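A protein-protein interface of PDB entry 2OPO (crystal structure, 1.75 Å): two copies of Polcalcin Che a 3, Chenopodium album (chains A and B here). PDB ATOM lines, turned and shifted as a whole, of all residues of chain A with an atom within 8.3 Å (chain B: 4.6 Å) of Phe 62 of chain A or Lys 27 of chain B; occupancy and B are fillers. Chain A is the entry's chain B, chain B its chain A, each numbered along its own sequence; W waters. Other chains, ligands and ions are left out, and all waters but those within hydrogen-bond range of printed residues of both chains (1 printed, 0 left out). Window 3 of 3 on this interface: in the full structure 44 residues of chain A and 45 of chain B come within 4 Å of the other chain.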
ATOM      1  N   MET A  52      -7.917 -28.194  18.163  1.00  0.00           N
ATOM      2  CA  MET A  52      -6.770 -27.292  17.985  1.00  0.00           C
ATOM      3  C   MET A  52      -6.931 -26.010  18.808  1.00  0.00           C
ATOM      4  O   MET A  52      -5.964 -25.519  19.403  1.00  0.00           O
ATOM      5  CB  MET A  52      -6.558 -26.908  16.533  1.00  0.00           C
ATOM      6  CG  MET A  52      -6.070 -28.044  15.646  1.00  0.00           C
ATOM      7  SD  MET A  52      -4.314 -28.535  15.938  1.00  0.00           S
ATOM      8  CE  MET A  52      -3.388 -27.068  15.655  1.00  0.00           C
ATOM      9  N   ILE A  55      -5.850 -26.519  22.435  1.00  0.00           N
ATOM     10  CA  ILE A  55      -4.456 -26.875  22.738  1.00  0.00           C
ATOM     11  C   ILE A  55      -3.433 -25.888  22.175  1.00  0.00           C
ATOM     12  O   ILE A  55      -2.464 -25.533  22.838  1.00  0.00           O
ATOM     13  CB  ILE A  55      -4.177 -28.340  22.246  1.00  0.00           C
ATOM     14  CG1 ILE A  55      -5.123 -29.326  22.933  1.00  0.00           C
ATOM     15  CG2 ILE A  55      -2.802 -28.781  22.630  1.00  0.00           C
ATOM     16  CD1 ILE A  55      -4.880 -30.781  22.493  1.00  0.00           C
ATOM     17  N   ASP A  56      -3.688 -25.394  20.958  1.00  0.00           N
ATOM     18  CA  ASP A  56      -2.902 -24.347  20.330  1.00  0.00           C
ATOM     19  C   ASP A  56      -3.265 -22.982  20.935  1.00  0.00           C
ATOM     20  O   ASP A  56      -4.012 -22.197  20.327  1.00  0.00           O
ATOM     21  CB  ASP A  56      -3.159 -24.334  18.818  1.00  0.00           C
ATOM     22  CG  ASP A  56      -2.563 -23.144  18.141  1.00  0.00           C
ATOM     23  OD1 ASP A  56      -1.615 -22.535  18.636  1.00  0.00           O
ATOM     24  OD2 ASP A  56      -3.063 -22.841  17.018  1.00  0.00           O
ATOM     25  N   THR A  57      -2.725 -22.715  22.130  1.00  0.00           N
ATOM     26  CA  THR A  57      -2.953 -21.485  22.867  1.00  0.00           C
ATOM     27  C   THR A  57      -2.566 -20.181  22.220  1.00  0.00           C
ATOM     28  O   THR A  57      -3.220 -19.149  22.469  1.00  0.00           O
ATOM     29  CB  THR A  57      -2.038 -21.468  24.131  1.00  0.00           C
ATOM     30  OG1 THR A  57      -2.131 -22.737  24.735  1.00  0.00           O
ATOM     31  CG2 THR A  57      -2.414 -20.347  25.075  1.00  0.00           C
ATOM     32  N   ASP A  58      -1.441 -20.184  21.519  1.00  0.00           N
ATOM     33  CA  ASP A  58      -0.918 -18.938  20.959  1.00  0.00           C
ATOM     34  C   ASP A  58      -1.495 -18.668  19.573  1.00  0.00           C
ATOM     35  O   ASP A  58      -1.216 -17.636  18.982  1.00  0.00           O
ATOM     36  CB  ASP A  58       0.609 -18.861  20.977  1.00  0.00           C
ATOM     37  CG  ASP A  58       1.297 -19.851  20.067  1.00  0.00           C
ATOM     38  OD1 ASP A  58       0.636 -20.534  19.262  1.00  0.00           O
ATOM     39  OD2 ASP A  58       2.565 -19.899  20.155  1.00  0.00           O
ATOM     40  N   GLY A  59      -2.274 -19.608  19.063  1.00  0.00           N
ATOM     41  CA  GLY A  59      -3.100 -19.355  17.887  1.00  0.00           C
ATOM     42  C   GLY A  59      -2.345 -19.410  16.578  1.00  0.00           C
ATOM     43  O   GLY A  59      -2.886 -19.044  15.507  1.00  0.00           O
ATOM     44  N   ASP A  60      -1.109 -19.908  16.630  1.00  0.00           N
ATOM     45  CA  ASP A  60      -0.262 -19.900  15.435  1.00  0.00           C
ATOM     46  C   ASP A  60      -0.655 -21.024  14.450  1.00  0.00           C
ATOM     47  O   ASP A  60      -0.160 -21.062  13.318  1.00  0.00           O
ATOM     48  CB  ASP A  60       1.230 -19.916  15.829  1.00  0.00           C
ATOM     49  CG  ASP A  60       1.718 -21.272  16.280  1.00  0.00           C
ATOM     50  OD1 ASP A  60       0.889 -22.145  16.591  1.00  0.00           O
ATOM     51  OD2 ASP A  60       2.950 -21.477  16.291  1.00  0.00           O
ATOM     52  N   GLY A  61      -1.560 -21.897  14.867  1.00  0.00           N
ATOM     53  CA  GLY A  61      -2.159 -22.914  13.996  1.00  0.00           C
ATOM     54  C   GLY A  61      -1.445 -24.243  14.173  1.00  0.00           C
ATOM     55  O   GLY A  61      -1.719 -25.198  13.462  1.00  0.00           O
ATOM     56  N   PHE A  62      -0.521 -24.301  15.129  1.00  0.00           N
ATOM     57  CA  PHE A  62       0.262 -25.522  15.389  1.00  0.00           C
ATOM     58  C   PHE A  62       0.259 -25.769  16.880  1.00  0.00           C
ATOM     59  O   PHE A  62       0.118 -24.815  17.667  1.00  0.00           O
ATOM     60  CB  PHE A  62       1.722 -25.393  14.956  1.00  0.00           C
ATOM     61  CG  PHE A  62       1.896 -25.252  13.503  1.00  0.00           C
ATOM     62  CD1 PHE A  62       1.961 -26.355  12.712  1.00  0.00           C
ATOM     63  CD2 PHE A  62       1.973 -24.009  12.935  1.00  0.00           C
ATOM     64  CE1 PHE A  62       2.084 -26.224  11.356  1.00  0.00           C
ATOM     65  CE2 PHE A  62       2.124 -23.873  11.572  1.00  0.00           C
ATOM     66  CZ  PHE A  62       2.206 -24.950  10.807  1.00  0.00           C
ATOM     67  N   ILE A  63       0.403 -27.037  17.243  1.00  0.00           N
ATOM     68  CA  ILE A  63       0.585 -27.425  18.632  1.00  0.00           C
ATOM     69  C   ILE A  63       2.076 -27.643  18.844  1.00  0.00           C
ATOM     70  O   ILE A  63       2.665 -28.554  18.255  1.00  0.00           O
ATOM     71  CB  ILE A  63      -0.180 -28.729  19.002  1.00  0.00           C
ATOM     72  CG1 ILE A  63      -1.690 -28.510  18.936  1.00  0.00           C
ATOM     73  CG2 ILE A  63       0.268 -29.208  20.384  1.00  0.00           C
ATOM     74  CD1 ILE A  63      -2.528 -29.759  18.980  1.00  0.00           C
ATOM     75  N   SER A  64       2.697 -26.781  19.655  1.00  0.00           N
ATOM     76  CA  SER A  64       4.080 -26.939  20.025  1.00  0.00           C
ATOM     77  C   SER A  64       4.232 -28.032  21.074  1.00  0.00           C
ATOM     78  O   SER A  64       3.299 -28.405  21.768  1.00  0.00           O
ATOM     79  CB  SER A  64       4.657 -25.630  20.559  1.00  0.00           C
ATOM     80  OG  SER A  64       3.968 -25.202  21.724  1.00  0.00           O
ATOM     81  N   PHE A  65       5.450 -28.516  21.232  1.00  0.00           N
ATOM     82  CA  PHE A  65       5.682 -29.471  22.303  1.00  0.00           C
ATOM     83  C   PHE A  65       5.353 -28.852  23.690  1.00  0.00           C
ATOM     84  O   PHE A  65       4.783 -29.530  24.574  1.00  0.00           O
ATOM     85  CB  PHE A  65       7.091 -30.013  22.212  1.00  0.00           C
ATOM     86  CG  PHE A  65       7.428 -30.932  23.309  1.00  0.00           C
ATOM     87  CD1 PHE A  65       6.990 -32.219  23.295  1.00  0.00           C
ATOM     88  CD2 PHE A  65       8.132 -30.470  24.397  1.00  0.00           C
ATOM     89  CE1 PHE A  65       7.267 -33.075  24.331  1.00  0.00           C
ATOM     90  CE2 PHE A  65       8.427 -31.320  25.431  1.00  0.00           C
ATOM     91  CZ  PHE A  65       7.988 -32.624  25.395  1.00  0.00           C
ATOM     92  N   ASP A  66       5.728 -27.578  23.908  1.00  0.00           N
ATOM     93  CA  ASP A  66       5.266 -26.857  25.115  1.00  0.00           C
ATOM     94  C   ASP A  66       3.749 -26.863  25.282  1.00  0.00           C
ATOM     95  O   ASP A  66       3.249 -27.117  26.383  1.00  0.00           O
ATOM     96  CB  ASP A  66       5.795 -25.417  25.139  1.00  0.00           C
ATOM     97  CG  ASP A  66       7.277 -25.384  25.323  1.00  0.00           C
ATOM     98  OD1 ASP A  66       7.831 -26.499  25.529  1.00  0.00           O
ATOM     99  OD2 ASP A  66       7.899 -24.280  25.291  1.00  0.00           O
ATOM    100  N   GLU A  67       3.010 -26.605  24.195  1.00  0.00           N
ATOM    101  CA  GLU A  67       1.553 -26.561  24.264  1.00  0.00           C
ATOM    102  C   GLU A  67       1.012 -27.953  24.575  1.00  0.00           C
ATOM    103  O   GLU A  67       0.078 -28.161  25.393  1.00  0.00           O
ATOM    104  CB  GLU A  67       0.977 -25.924  22.967  1.00  0.00           C
ATOM    105  CG  GLU A  67       1.165 -24.370  22.905  1.00  0.00           C
ATOM    106  CD  GLU A  67       0.794 -23.733  21.542  1.00  0.00           C
ATOM    107  OE1 GLU A  67       0.931 -24.414  20.549  1.00  0.00           O
ATOM    108  OE2 GLU A  67       0.479 -22.520  21.467  1.00  0.00           O
ATOM    109  N   PHE A  68       1.622 -28.956  23.963  1.00  0.00           N
ATOM    110  CA  PHE A  68       1.213 -30.318  24.200  1.00  0.00           C
ATOM    111  C   PHE A  68       1.482 -30.714  25.652  1.00  0.00           C
ATOM    112  O   PHE A  68       0.664 -31.398  26.301  1.00  0.00           O
ATOM    113  CB  PHE A  68       1.960 -31.272  23.278  1.00  0.00           C
ATOM    114  CG  PHE A  68       1.572 -32.676  23.484  1.00  0.00           C
ATOM    115  CD1 PHE A  68       0.336 -33.112  23.080  1.00  0.00           C
ATOM    116  CD2 PHE A  68       2.432 -33.550  24.124  1.00  0.00           C
ATOM    117  CE1 PHE A  68      -0.038 -34.417  23.295  1.00  0.00           C
ATOM    118  CE2 PHE A  68       2.074 -34.863  24.291  1.00  0.00           C
ATOM    119  CZ  PHE A  68       0.852 -35.282  23.915  1.00  0.00           C
ATOM    120  N   PHE B  17       3.748 -37.534  21.346  1.00  0.00           N
ATOM    121  CA  PHE B  17       3.999 -36.342  20.508  1.00  0.00           C
ATOM    122  C   PHE B  17       4.688 -36.769  19.205  1.00  0.00           C
ATOM    123  O   PHE B  17       4.270 -36.408  18.094  1.00  0.00           O
ATOM    124  CB  PHE B  17       4.842 -35.292  21.250  1.00  0.00           C
ATOM    125  CG  PHE B  17       4.981 -33.978  20.515  1.00  0.00           C
ATOM    126  CD1 PHE B  17       4.077 -32.954  20.706  1.00  0.00           C
ATOM    127  CD2 PHE B  17       6.036 -33.755  19.650  1.00  0.00           C
ATOM    128  CE1 PHE B  17       4.184 -31.760  20.022  1.00  0.00           C
ATOM    129  CE2 PHE B  17       6.167 -32.552  18.987  1.00  0.00           C
ATOM    130  CZ  PHE B  17       5.244 -31.549  19.173  1.00  0.00           C
ATOM    131  N   ASP B  21       3.371 -36.290  15.446  1.00  0.00           N
ATOM    132  CA  ASP B  21       4.176 -35.401  14.594  1.00  0.00           C
ATOM    133  C   ASP B  21       4.867 -36.260  13.545  1.00  0.00           C
ATOM    134  O   ASP B  21       6.089 -36.561  13.613  1.00  0.00           O
ATOM    135  CB  ASP B  21       5.175 -34.600  15.415  1.00  0.00           C
ATOM    136  CG  ASP B  21       6.109 -33.724  14.544  1.00  0.00           C
ATOM    137  OD1 ASP B  21       5.664 -33.255  13.457  1.00  0.00           O
ATOM    138  OD2 ASP B  21       7.244 -33.516  14.990  1.00  0.00           O
ATOM    139  N   ASP B  25       8.785 -32.355  12.245  1.00  0.00           N
ATOM    140  CA  ASP B  25       9.237 -30.955  12.272  1.00  0.00           C
ATOM    141  C   ASP B  25       9.157 -30.273  13.669  1.00  0.00           C
ATOM    142  O   ASP B  25       9.587 -29.101  13.838  1.00  0.00           O
ATOM    143  CB  ASP B  25       8.541 -30.118  11.197  1.00  0.00           C
ATOM    144  CG  ASP B  25       7.110 -29.875  11.483  1.00  0.00           C
ATOM    145  OD1 ASP B  25       6.600 -30.499  12.437  1.00  0.00           O
ATOM    146  OD2 ASP B  25       6.496 -29.130  10.672  1.00  0.00           O
ATOM    147  N   GLY B  26       8.738 -31.050  14.660  1.00  0.00           N
ATOM    148  CA  GLY B  26       8.682 -30.594  16.051  1.00  0.00           C
ATOM    149  C   GLY B  26       7.373 -29.953  16.496  1.00  0.00           C
ATOM    150  O   GLY B  26       7.281 -29.500  17.601  1.00  0.00           O
ATOM    151  N   LYS B  27       6.388 -29.869  15.610  1.00  0.00           N
ATOM    152  CA  LYS B  27       5.099 -29.286  15.900  1.00  0.00           C
ATOM    153  C   LYS B  27       3.951 -30.098  15.263  1.00  0.00           C
ATOM    154  O   LYS B  27       4.162 -30.836  14.306  1.00  0.00           O
ATOM    155  CB  LYS B  27       5.036 -27.855  15.459  1.00  0.00           C
ATOM    156  CG  LYS B  27       5.302 -27.626  13.995  1.00  0.00           C
ATOM    157  CD  LYS B  27       5.489 -26.142  13.735  1.00  0.00           C
ATOM    158  CE  LYS B  27       5.564 -25.843  12.244  1.00  0.00           C
ATOM    159  NZ  LYS B  27       6.316 -24.594  11.955  1.00  0.00           N
ATOM    160  N   ILE B  28       2.740 -29.984  15.802  1.00  0.00           N
ATOM    161  CA  ILE B  28       1.571 -30.768  15.273  1.00  0.00           C
ATOM    162  C   ILE B  28       0.638 -29.824  14.535  1.00  0.00           C
ATOM    163  O   ILE B  28       0.078 -28.889  15.124  1.00  0.00           O
ATOM    164  CB  ILE B  28       0.821 -31.571  16.401  1.00  0.00           C
ATOM    165  CG1 ILE B  28       1.821 -32.460  17.144  1.00  0.00           C
ATOM    166  CG2 ILE B  28      -0.421 -32.286  15.866  1.00  0.00           C
ATOM    167  CD1 ILE B  28       1.252 -33.112  18.442  1.00  0.00           C
ATOM    168  N   SER B  29       0.454 -30.059  13.236  1.00  0.00           N
ATOM    169  CA  SER B  29      -0.471 -29.269  12.451  1.00  0.00           C
ATOM    170  C   SER B  29      -1.897 -29.768  12.643  1.00  0.00           C
ATOM    171  O   SER B  29      -2.133 -30.862  13.191  1.00  0.00           O
ATOM    172  CB  SER B  29      -0.100 -29.386  10.963  1.00  0.00           C
ATOM    173  OG  SER B  29      -0.280 -30.740  10.568  1.00  0.00           O
ATOM    174  N   GLU B  32      -2.146 -33.137  10.962  1.00  0.00           N
ATOM    175  CA  GLU B  32      -1.509 -34.159  11.803  1.00  0.00           C
ATOM    176  C   GLU B  32      -2.451 -34.602  12.972  1.00  0.00           C
ATOM    177  O   GLU B  32      -2.633 -35.820  13.249  1.00  0.00           O
ATOM    178  CB  GLU B  32      -0.164 -33.636  12.303  1.00  0.00           C
ATOM    179  CG  GLU B  32       0.986 -33.817  11.266  1.00  0.00           C
ATOM    180  CD  GLU B  32       2.260 -33.172  11.667  1.00  0.00           C
ATOM    181  OE1 GLU B  32       2.262 -32.282  12.533  1.00  0.00           O
ATOM    182  OE2 GLU B  32       3.308 -33.530  11.084  1.00  0.00           O
HETATM  183  O   HOH W   1       7.625 -27.625  19.395  1.00  0.00           O
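OG of Ser 29 of chain B is in hydrogen-bond range of N of Glu 32 of chain B (3.1 Å).
The backbone NH of Glu 67 of chain A lies within hydrogen-bond range of the side-chain hydroxyl of Ser 64 of chain A, 3.0 Å away.
O of Ile 28 of chain B is in hydrogen-bond range of N of Ile 63 of chain A, at 2.8 Å.
Water W1 bridges the backbone carbonyl oxygen of Gly 26 of chain B (2.6 Å) and the backbone NH of Phe 65 of chain A (3.0 Å).
No position is printed for both chains.
Of the 8 printed residues of chain B, 4 touch a printed residue of chain A.
Printed residues of chain B that touch a printed residue of chain A: Phe 17, Lys 27, Ile 28 and Ser 29.
Hydrophobic or aromatic side chains of chain B within 4 Å of the printed part of chain A: Phe 17 and Ile 28.
Hydrophobic or aromatic side chains of chain A that line the printed part of chain B: Met 52, Phe 62, Ile 63, Phe 65 and Phe 68.
Phe 62 of chain A touches just these residues of chain B: Lys 27, Ile 28 and Ser 29.
Lys 27 of chain B touches two residues of chain A.
No residue of chain A comes within 4 Å of Gly 26 of chain B.
Of the printed residues of chain A, Phe 17 of chain B touches Ile 63 (3.96 Å), Ser 64 (3.9 Å), Phe 65 (3.6 Å) and Phe 68 (3.7 Å).
Of the printed residues of chain B, Phe 68 of chain A touches Phe 17 (3.7 Å).
Gly 59 of chain A touches none of the printed residues of chain B.
The nearest residue of chain A that does not touch Lys 27 of chain B is Ser 64 of chain A (4.8 Å).
Among the printed residues, pairs that only touch across the chains: Phe 62 of chain A with Ile 28 of chain B (3.4 Å), Ile 63 of chain A with Lys 27 of chain B (3.5 Å), Phe 65 of chain A with Phe 17 of chain B (3.6 Å), Phe 62 of chain A with Lys 27 of chain B (3.6 Å), Phe 68 of chain A with Phe 17 of chain B (3.7 Å), Phe 62 of chain A with Ser 29 of chain B (3.8 Å), Ser 64 of chain A with Phe 17 of chain B (3.9 Å), Met 52 of chain A with Ile 28 of chain B (3.95 Å) and Ile 63 of chain A with Phe 17 of chain B (3.96 Å).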
